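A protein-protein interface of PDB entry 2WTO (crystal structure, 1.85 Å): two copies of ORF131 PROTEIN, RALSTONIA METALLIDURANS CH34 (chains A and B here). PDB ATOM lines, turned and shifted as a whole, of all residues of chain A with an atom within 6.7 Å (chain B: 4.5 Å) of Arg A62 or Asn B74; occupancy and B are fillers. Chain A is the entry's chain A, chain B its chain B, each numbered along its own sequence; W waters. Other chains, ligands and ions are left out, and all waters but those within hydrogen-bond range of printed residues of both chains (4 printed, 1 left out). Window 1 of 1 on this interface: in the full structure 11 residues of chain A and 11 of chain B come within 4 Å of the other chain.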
ATOM      1  N   GLN A  57      -9.167  11.987 -14.128  1.00  0.00           N
ATOM      2  CA  GLN A  57      -9.920  13.220 -13.911  1.00  0.00           C
ATOM      3  C   GLN A  57     -11.431  13.075 -14.136  1.00  0.00           C
ATOM      4  O   GLN A  57     -12.250  13.748 -13.483  1.00  0.00           O
ATOM      5  CB  GLN A  57      -9.375  14.291 -14.859  1.00  0.00           C
ATOM      6  CG  GLN A  57      -9.896  15.668 -14.538  1.00  0.00           C
ATOM      7  CD  GLN A  57      -9.648  16.654 -15.657  1.00  0.00           C
ATOM      8  OE1 GLN A  57      -8.648  16.548 -16.395  1.00  0.00           O
ATOM      9  NE2 GLN A  57     -10.559  17.628 -15.792  1.00  0.00           N
ATOM     10  N   GLN A  59     -13.346  10.868 -13.267  1.00  0.00           N
ATOM     11  CA  GLN A  59     -14.060  10.257 -12.154  1.00  0.00           C
ATOM     12  C   GLN A  59     -14.000  11.119 -10.886  1.00  0.00           C
ATOM     13  O   GLN A  59     -14.565  10.757  -9.860  1.00  0.00           O
ATOM     14  CB  GLN A  59     -13.533   8.849 -11.869  1.00  0.00           C
ATOM     15  CG  GLN A  59     -13.950   7.815 -12.925  1.00  0.00           C
ATOM     16  CD  GLN A  59     -15.453   7.551 -12.928  1.00  0.00           C
ATOM     17  OE1 GLN A  59     -16.019   7.156 -11.917  1.00  0.00           O
ATOM     18  NE2 GLN A  59     -16.097   7.742 -14.082  1.00  0.00           N
ATOM     19  N   ALA A  60     -13.339  12.271 -10.979  1.00  0.00           N
ATOM     20  CA  ALA A  60     -13.145  13.119  -9.802  1.00  0.00           C
ATOM     21  C   ALA A  60     -14.410  13.928  -9.484  1.00  0.00           C
ATOM     22  O   ALA A  60     -15.074  14.438 -10.399  1.00  0.00           O
ATOM     23  CB  ALA A  60     -11.968  14.062 -10.014  1.00  0.00           C
ATOM     24  N   SER A  61     -14.721  14.063  -8.196  1.00  0.00           N
ATOM     25  CA  SER A  61     -15.887  14.847  -7.771  1.00  0.00           C
ATOM     26  C   SER A  61     -15.614  16.345  -7.568  1.00  0.00           C
ATOM     27  O   SER A  61     -16.546  17.120  -7.388  1.00  0.00           O
ATOM     28  CB  SER A  61     -16.515  14.248  -6.510  1.00  0.00           C
ATOM     29  OG  SER A  61     -15.530  14.070  -5.503  1.00  0.00           O
ATOM     30  N   ARG A  62     -14.349  16.736  -7.565  1.00  0.00           N
ATOM     31  CA  ARG A  62     -13.973  18.139  -7.504  1.00  0.00           C
ATOM     32  C   ARG A  62     -12.533  18.283  -7.995  1.00  0.00           C
ATOM     33  O   ARG A  62     -11.773  17.300  -8.075  1.00  0.00           O
ATOM     34  CB  ARG A  62     -14.097  18.702  -6.081  1.00  0.00           C
ATOM     35  CG  ARG A  62     -13.196  17.987  -5.054  1.00  0.00           C
ATOM     36  CD  ARG A  62     -13.177  18.737  -3.714  1.00  0.00           C
ATOM     37  NE  ARG A  62     -12.799  17.849  -2.612  1.00  0.00           N
ATOM     38  CZ  ARG A  62     -12.257  18.262  -1.469  1.00  0.00           C
ATOM     39  NH1 ARG A  62     -12.008  19.554  -1.280  1.00  0.00           N
ATOM     40  NH2 ARG A  62     -11.971  17.373  -0.516  1.00  0.00           N
ATOM     41  N   ILE A  63     -12.165  19.511  -8.329  1.00  0.00           N
ATOM     42  CA  ILE A  63     -10.785  19.810  -8.714  1.00  0.00           C
ATOM     43  C   ILE A  63     -10.234  20.818  -7.718  1.00  0.00           C
ATOM     44  O   ILE A  63     -10.831  21.876  -7.494  1.00  0.00           O
ATOM     45  CB  ILE A  63     -10.704  20.397 -10.134  1.00  0.00           C
ATOM     46  CG1 ILE A  63     -11.193  19.378 -11.169  1.00  0.00           C
ATOM     47  CG2 ILE A  63      -9.289  20.810 -10.451  1.00  0.00           C
ATOM     48  CD1 ILE A  63     -11.463  19.983 -12.551  1.00  0.00           C
ATOM     49  N   ILE A  64      -9.103  20.490  -7.106  1.00  0.00           N
ATOM     50  CA  ILE A  64      -8.504  21.388  -6.114  1.00  0.00           C
ATOM     51  C   ILE A  64      -7.315  22.130  -6.723  1.00  0.00           C
ATOM     52  O   ILE A  64      -6.364  21.518  -7.235  1.00  0.00           O
ATOM     53  CB  ILE A  64      -8.068  20.616  -4.835  1.00  0.00           C
ATOM     54  CG1 ILE A  64      -9.287  20.006  -4.130  1.00  0.00           C
ATOM     55  CG2 ILE A  64      -7.305  21.558  -3.881  1.00  0.00           C
ATOM     56  CD1 ILE A  64      -8.975  19.267  -2.851  1.00  0.00           C
ATOM     57  N   TYR A  72      -2.712  22.648   3.609  1.00  0.00           N
ATOM     58  CA  TYR A  72      -3.445  21.382   3.674  1.00  0.00           C
ATOM     59  C   TYR A  72      -4.799  21.424   3.004  1.00  0.00           C
ATOM     60  O   TYR A  72      -5.329  22.507   2.718  1.00  0.00           O
ATOM     61  CB  TYR A  72      -3.601  20.857   5.108  1.00  0.00           C
ATOM     62  CG  TYR A  72      -4.616  21.589   5.976  1.00  0.00           C
ATOM     63  CD1 TYR A  72      -5.957  21.205   5.999  1.00  0.00           C
ATOM     64  CD2 TYR A  72      -4.214  22.634   6.802  1.00  0.00           C
ATOM     65  CE1 TYR A  72      -6.896  21.883   6.826  1.00  0.00           C
ATOM     66  CE2 TYR A  72      -5.120  23.294   7.624  1.00  0.00           C
ATOM     67  CZ  TYR A  72      -6.451  22.919   7.634  1.00  0.00           C
ATOM     68  OH  TYR A  72      -7.315  23.603   8.468  1.00  0.00           O
ATOM     69  N   VAL A  73      -5.329  20.232   2.738  1.00  0.00           N
ATOM     70  CA  VAL A  73      -6.705  20.056   2.280  1.00  0.00           C
ATOM     71  C   VAL A  73      -7.281  18.849   3.013  1.00  0.00           C
ATOM     72  O   VAL A  73      -6.525  18.036   3.524  1.00  0.00           O
ATOM     73  CB  VAL A  73      -6.796  19.848   0.728  1.00  0.00           C
ATOM     74  CG1 VAL A  73      -6.143  21.013  -0.002  1.00  0.00           C
ATOM     75  CG2 VAL A  73      -6.138  18.551   0.315  1.00  0.00           C
ATOM     76  N   ASN A  74      -8.608  18.750   3.093  1.00  0.00           N
ATOM     77  CA  ASN A  74      -9.263  17.618   3.743  1.00  0.00           C
ATOM     78  C   ASN A  74      -9.918  16.784   2.653  1.00  0.00           C
ATOM     79  O   ASN A  74     -10.676  17.316   1.846  1.00  0.00           O
ATOM     80  CB  ASN A  74     -10.372  18.084   4.686  1.00  0.00           C
ATOM     81  CG  ASN A  74      -9.841  18.797   5.918  1.00  0.00           C
ATOM     82  OD1 ASN A  74      -8.664  18.684   6.252  1.00  0.00           O
ATOM     83  ND2 ASN A  74     -10.718  19.508   6.615  1.00  0.00           N
ATOM     84  N   VAL A  75      -9.640  15.484   2.642  1.00  0.00           N
ATOM     85  CA  VAL A  75     -10.353  14.565   1.748  1.00  0.00           C
ATOM     86  C   VAL A  75     -10.955  13.412   2.563  1.00  0.00           C
ATOM     87  O   VAL A  75     -10.537  13.154   3.697  1.00  0.00           O
ATOM     88  CB  VAL A  75      -9.430  14.034   0.635  1.00  0.00           C
ATOM     89  CG1 VAL A  75      -8.820  15.207  -0.162  1.00  0.00           C
ATOM     90  CG2 VAL A  75      -8.337  13.095   1.232  1.00  0.00           C
ATOM     91  N   ASP A  76     -11.970  12.748   2.001  1.00  0.00           N
ATOM     92  CA  ASP A  76     -12.555  11.575   2.636  1.00  0.00           C
ATOM     93  C   ASP A  76     -11.863  10.292   2.169  1.00  0.00           C
ATOM     94  O   ASP A  76     -11.374  10.222   1.055  1.00  0.00           O
ATOM     95  CB  ASP A  76     -14.044  11.482   2.297  1.00  0.00           C
ATOM     96  CG  ASP A  76     -14.891  12.385   3.183  1.00  0.00           C
ATOM     97  OD1 ASP A  76     -14.524  12.558   4.362  1.00  0.00           O
ATOM     98  OD2 ASP A  76     -15.912  12.917   2.707  1.00  0.00           O
ATOM     99  N   GLU A  79     -12.588   9.090  -1.476  1.00  0.00           N
ATOM    100  CA  GLU A  79     -12.862  10.224  -2.366  1.00  0.00           C
ATOM    101  C   GLU A  79     -11.916  10.237  -3.554  1.00  0.00           C
ATOM    102  O   GLU A  79     -10.722   9.933  -3.423  1.00  0.00           O
ATOM    103  CB  GLU A  79     -12.776  11.544  -1.578  1.00  0.00           C
ATOM    104  CG  GLU A  79     -13.321  12.759  -2.319  1.00  0.00           C
ATOM    105  CD  GLU A  79     -13.177  14.053  -1.516  1.00  0.00           C
ATOM    106  OE1 GLU A  79     -12.757  14.000  -0.339  1.00  0.00           O
ATOM    107  OE2 GLU A  79     -13.527  15.124  -2.064  1.00  0.00           O
ATOM    108  N   THR A  80     -12.460  10.539  -4.734  1.00  0.00           N
ATOM    109  CA  THR A  80     -11.661  10.751  -5.921  1.00  0.00           C
ATOM    110  C   THR A  80     -11.580  12.253  -6.214  1.00  0.00           C
ATOM    111  O   THR A  80     -12.592  12.917  -6.483  1.00  0.00           O
ATOM    112  CB  THR A  80     -12.198   9.973  -7.163  1.00  0.00           C
ATOM    113  OG1 THR A  80     -12.209   8.559  -6.874  1.00  0.00           O
ATOM    114  CG2 THR A  80     -11.289  10.247  -8.359  1.00  0.00           C
ATOM    115  N   VAL A  81     -10.359  12.774  -6.137  1.00  0.00           N
ATOM    116  CA  VAL A  81     -10.112  14.212  -6.174  1.00  0.00           C
ATOM    117  C   VAL A  81      -9.075  14.525  -7.221  1.00  0.00           C
ATOM    118  O   VAL A  81      -8.037  13.863  -7.274  1.00  0.00           O
ATOM    119  CB  VAL A  81      -9.582  14.723  -4.794  1.00  0.00           C
ATOM    120  CG1 VAL A  81      -9.309  16.230  -4.866  1.00  0.00           C
ATOM    121  CG2 VAL A  81     -10.568  14.405  -3.704  1.00  0.00           C
ATOM    122  N   ALA A  82      -9.335  15.540  -8.050  1.00  0.00           N
ATOM    123  CA  ALA A  82      -8.330  16.006  -8.991  1.00  0.00           C
ATOM    124  C   ALA A  82      -7.621  17.228  -8.441  1.00  0.00           C
ATOM    125  O   ALA A  82      -8.236  18.063  -7.757  1.00  0.00           O
ATOM    126  CB  ALA A  82      -8.962  16.315 -10.373  1.00  0.00           C
ATOM    127  N   PHE A  83      -6.322  17.311  -8.717  1.00  0.00           N
ATOM    128  CA  PHE A  83      -5.505  18.406  -8.233  1.00  0.00           C
ATOM    129  C   PHE A  83      -4.939  19.109  -9.441  1.00  0.00           C
ATOM    130  O   PHE A  83      -4.394  18.479 -10.354  1.00  0.00           O
ATOM    131  CB  PHE A  83      -4.381  17.880  -7.328  1.00  0.00           C
ATOM    132  CG  PHE A  83      -4.889  17.273  -6.044  1.00  0.00           C
ATOM    133  CD1 PHE A  83      -5.040  18.057  -4.910  1.00  0.00           C
ATOM    134  CD2 PHE A  83      -5.258  15.920  -5.992  1.00  0.00           C
ATOM    135  CE1 PHE A  83      -5.533  17.495  -3.697  1.00  0.00           C
ATOM    136  CE2 PHE A  83      -5.762  15.350  -4.818  1.00  0.00           C
ATOM    137  CZ  PHE A  83      -5.901  16.143  -3.660  1.00  0.00           C
ATOM    138  N   ARG B  62      -6.368  27.737   7.918  1.00  0.00           N
ATOM    139  CA  ARG B  62      -6.083  27.840   6.484  1.00  0.00           C
ATOM    140  C   ARG B  62      -7.011  28.859   5.854  1.00  0.00           C
ATOM    141  O   ARG B  62      -8.083  29.161   6.408  1.00  0.00           O
ATOM    142  CB  ARG B  62      -6.258  26.486   5.777  1.00  0.00           C
ATOM    143  CG  ARG B  62      -7.648  25.868   5.988  1.00  0.00           C
ATOM    144  CD  ARG B  62      -7.890  24.733   4.995  1.00  0.00           C
ATOM    145  NE  ARG B  62      -9.006  23.919   5.434  1.00  0.00           N
ATOM    146  CZ  ARG B  62      -9.688  23.067   4.671  1.00  0.00           C
ATOM    147  NH1 ARG B  62      -9.385  22.884   3.383  1.00  0.00           N
ATOM    148  NH2 ARG B  62     -10.662  22.375   5.231  1.00  0.00           N
ATOM    149  N   MET B  70     -16.191  25.573  -7.852  1.00  0.00           N
ATOM    150  CA  MET B  70     -15.341  24.693  -7.011  1.00  0.00           C
ATOM    151  C   MET B  70     -16.107  23.511  -6.384  1.00  0.00           C
ATOM    152  O   MET B  70     -15.494  22.546  -5.888  1.00  0.00           O
ATOM    153  CB  MET B  70     -14.619  25.487  -5.924  1.00  0.00           C
ATOM    154  CG  MET B  70     -15.522  25.950  -4.809  1.00  0.00           C
ATOM    155  SD  MET B  70     -14.646  27.034  -3.645  1.00  0.00           S
ATOM    156  CE  MET B  70     -13.170  26.097  -3.251  1.00  0.00           C
ATOM    157  N   TYR B  72     -17.427  21.984  -3.772  1.00  0.00           N
ATOM    158  CA  TYR B  72     -17.514  21.816  -2.321  1.00  0.00           C
ATOM    159  C   TYR B  72     -16.163  21.869  -1.644  1.00  0.00           C
ATOM    160  O   TYR B  72     -15.128  21.809  -2.296  1.00  0.00           O
ATOM    161  CB  TYR B  72     -18.203  20.502  -1.942  1.00  0.00           C
ATOM    162  CG  TYR B  72     -17.438  19.241  -2.362  1.00  0.00           C
ATOM    163  CD1 TYR B  72     -16.566  18.590  -1.469  1.00  0.00           C
ATOM    164  CD2 TYR B  72     -17.586  18.714  -3.637  1.00  0.00           C
ATOM    165  CE1 TYR B  72     -15.871  17.427  -1.852  1.00  0.00           C
ATOM    166  CE2 TYR B  72     -16.899  17.550  -4.038  1.00  0.00           C
ATOM    167  CZ  TYR B  72     -16.048  16.915  -3.140  1.00  0.00           C
ATOM    168  OH  TYR B  72     -15.377  15.770  -3.535  1.00  0.00           O
ATOM    169  N   VAL B  73     -16.194  22.004  -0.320  1.00  0.00           N
ATOM    170  CA  VAL B  73     -14.991  21.837   0.503  1.00  0.00           C
ATOM    171  C   VAL B  73     -15.339  20.892   1.637  1.00  0.00           C
ATOM    172  O   VAL B  73     -16.525  20.704   1.937  1.00  0.00           O
ATOM    173  CB  VAL B  73     -14.495  23.184   1.099  1.00  0.00           C
ATOM    174  CG1 VAL B  73     -14.151  24.144  -0.006  1.00  0.00           C
ATOM    175  CG2 VAL B  73     -15.555  23.794   2.031  1.00  0.00           C
ATOM    176  N   ASN B  74     -14.315  20.299   2.267  1.00  0.00           N
ATOM    177  CA  ASN B  74     -14.507  19.433   3.422  1.00  0.00           C
ATOM    178  C   ASN B  74     -13.883  20.118   4.638  1.00  0.00           C
ATOM    179  O   ASN B  74     -12.726  20.540   4.583  1.00  0.00           O
ATOM    180  CB  ASN B  74     -13.808  18.063   3.246  1.00  0.00           C
ATOM    181  CG  ASN B  74     -14.508  17.139   2.244  1.00  0.00           C
ATOM    182  OD1 ASN B  74     -15.654  17.354   1.864  1.00  0.00           O
ATOM    183  ND2 ASN B  74     -13.805  16.084   1.827  1.00  0.00           N
ATOM    184  N   VAL B  75     -14.633  20.212   5.728  1.00  0.00           N
ATOM    185  CA  VAL B  75     -14.094  20.783   6.967  1.00  0.00           C
ATOM    186  C   VAL B  75     -14.392  19.875   8.149  1.00  0.00           C
ATOM    187  O   VAL B  75     -15.337  19.083   8.118  1.00  0.00           O
ATOM    188  CB  VAL B  75     -14.668  22.191   7.261  1.00  0.00           C
ATOM    189  CG1 VAL B  75     -14.445  23.103   6.077  1.00  0.00           C
ATOM    190  CG2 VAL B  75     -16.182  22.098   7.609  1.00  0.00           C
ATOM    191  N   GLU B  79     -12.988  22.951  13.296  1.00  0.00           N
ATOM    192  CA  GLU B  79     -11.979  23.604  12.460  1.00  0.00           C
ATOM    193  C   GLU B  79     -12.324  25.087  12.241  1.00  0.00           C
ATOM    194  O   GLU B  79     -13.498  25.438  12.070  1.00  0.00           O
ATOM    195  CB  GLU B  79     -11.863  22.881  11.108  1.00  0.00           C
ATOM    196  CG  GLU B  79     -10.630  23.278  10.273  1.00  0.00           C
ATOM    197  CD  GLU B  79     -10.615  22.637   8.880  1.00  0.00           C
ATOM    198  OE1 GLU B  79     -11.422  21.706   8.651  1.00  0.00           O
ATOM    199  OE2 GLU B  79      -9.793  23.057   8.035  1.00  0.00           O
ATOM    200  N   TYR B 121     -19.028  20.281   3.488  1.00  0.00           N
ATOM    201  CA  TYR B 121     -19.253  19.019   4.185  1.00  0.00           C
ATOM    202  C   TYR B 121     -18.507  19.046   5.505  1.00  0.00           C
ATOM    203  O   TYR B 121     -17.285  19.139   5.503  1.00  0.00           O
ATOM    204  CB  TYR B 121     -18.779  17.822   3.337  1.00  0.00           C
ATOM    205  CG  TYR B 121     -19.676  17.588   2.143  1.00  0.00           C
ATOM    206  CD1 TYR B 121     -20.840  16.826   2.261  1.00  0.00           C
ATOM    207  CD2 TYR B 121     -19.370  18.141   0.909  1.00  0.00           C
ATOM    208  CE1 TYR B 121     -21.676  16.620   1.171  1.00  0.00           C
ATOM    209  CE2 TYR B 121     -20.208  17.945  -0.196  1.00  0.00           C
ATOM    210  CZ  TYR B 121     -21.361  17.188  -0.047  1.00  0.00           C
ATOM    211  OH  TYR B 121     -22.191  16.994  -1.135  1.00  0.00           O
HETATM  212  O   HOH W   1     -12.535  22.657  -5.484  1.00  0.00           O
HETATM  213  O   HOH W   2      -7.231  24.104   1.725  1.00  0.00           O
HETATM  214  O   HOH W   3     -12.488  22.071  -2.734  1.00  0.00           O
HETATM  215  O   HOH W   4     -17.246  15.293   1.090  1.00  0.00           O
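Arg A62 touches Tyr B72, and with the chains exchanged Tyr A72 touches Arg B62. Arg A62 touches Asn B74, and with the chains exchanged Asn A74 touches Arg B62. Asn B74 touches its own counterpart, Asn A74. Asn A74 touches Val B75, and with the chains exchanged Val A75 touches Asn B74. Positions printed for both chains: 62, 72, 73, 74, 75 and 79. Of the 13 pairs that touch across the chains among the printed residues, 11 have their exchanged pair printed and touching as well.
Printed residues of chain B within 4 Å of Ser A61: Tyr B72. Of the printed residues of chain B, Asn A74 touches Arg B62, Asn B74, Val B75 and Glu B79. Printed residues of chain A within 4 Å of Arg B62: Tyr A72 and Asn A74. Asn B74 touches just these residues of chain A: Arg A62 (3.2 Å), Asn A74 (3.0 Å), Val A75 (3.8 Å), Asp A76 (3.8 Å) and Glu A79 (3.2 Å). The nearest printed residue of chain A that does not touch Asn B74 is Val A73 (5.9 Å). The nearest printed residue of chain A that does not touch Val B75 is Tyr A72 (7.3 Å).
OH of Tyr A72 sits close to NE of Arg B62, at 3.5 Å. The guanidinium group of Arg A62 sits close to the side-chain hydroxyl of Tyr B72 (3.4 Å). OG of Ser A61 lies within hydrogen-bond range of OH of Tyr B72 (2.6 Å). OH of Tyr B72 is in hydrogen-bond range of OE2 of Glu A79, at 2.5 Å. The side-chain carboxylate (OE2) of Glu B79 is in hydrogen-bond range of the side-chain hydroxyl (OH) of Tyr A72 (2.6 Å). The guanidinium group (NH2) of Arg A62 sits close to the side-chain amide nitrogen (ND2) of Asn B74. The side-chain amide nitrogen of Asn A74 sits at hydrogen-bond distance from the side-chain carboxylate of Glu B79, at 3.1 Å. OE1 of Glu A79 is in hydrogen-bond range of ND2 of Asn B74 (3.2 Å). The side-chain amide nitrogen (ND2) of Asn A74 sits close to the guanidinium group (NH2) of Arg B62 (3.2 Å). The backbone carbonyl oxygen (O) of Asn B74 is in hydrogen-bond range of the side-chain amide nitrogen (ND2) of Asn A74, 3.0 Å away.
N of Asp A76 is in hydrogen-bond range of OE1 of Glu A79 (2.8 Å). NE of Arg A62 is in salt-bridge range of OE2 of Glu A79, 2.9 Å away. The guanidinium group (NH2) of Arg A62 lies within hydrogen-bond range of the backbone carbonyl oxygen (O) of Asn A74 (2.7 Å). The guanidinium group of Arg B62 is in salt-bridge range of the side-chain carboxylate of Glu B79 (2.9 Å). The guanidinium group (NH2) of Arg B62 sits at hydrogen-bond distance from the backbone carbonyl oxygen (O) of Asn B74 (2.8 Å). The backbone carbonyl oxygen (O) of Tyr B121 lies within hydrogen-bond range of the backbone NH (N) of Val B75, at 2.9 Å.
Hydrophobic or aromatic side chains of chain B that line the printed part of chain A: Tyr B72. Of the 17 printed residues of chain A, 7 touch a printed residue of chain B. Hydrophobic or aromatic side chains of chain A within 4 Å of the printed part of chain B: Tyr A72. Among the printed residues, 13 pairs touch across the chains. Among the printed residues, no Asp or Glu carboxylate lies within 4 Å of a Lys or Arg side-chain nitrogen of the other chain.
Asn A74 touches Val B75. Val A75 touches Asn B74. Asp A76 touches Asn B74 (N to ND2, 3.8 Å).
Water W2 bridges the backbone carbonyl oxygen (O) of Tyr A72 (2.7 Å) and the guanidinium group (NH1) of Arg B62 (3.0 Å). Water W3 lies within hydrogen-bond range of O of Tyr B72 (2.7 Å) and NH1 of Arg A62 (2.9 Å). Water W4 lies within hydrogen-bond range of OD1 of Asn B74 (2.7 Å) and OD2 of Asp A76 (3.2 Å). Water W1 bridges O of Ile A63 (2.7 Å) and O of Met B70 (3.0 Å).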
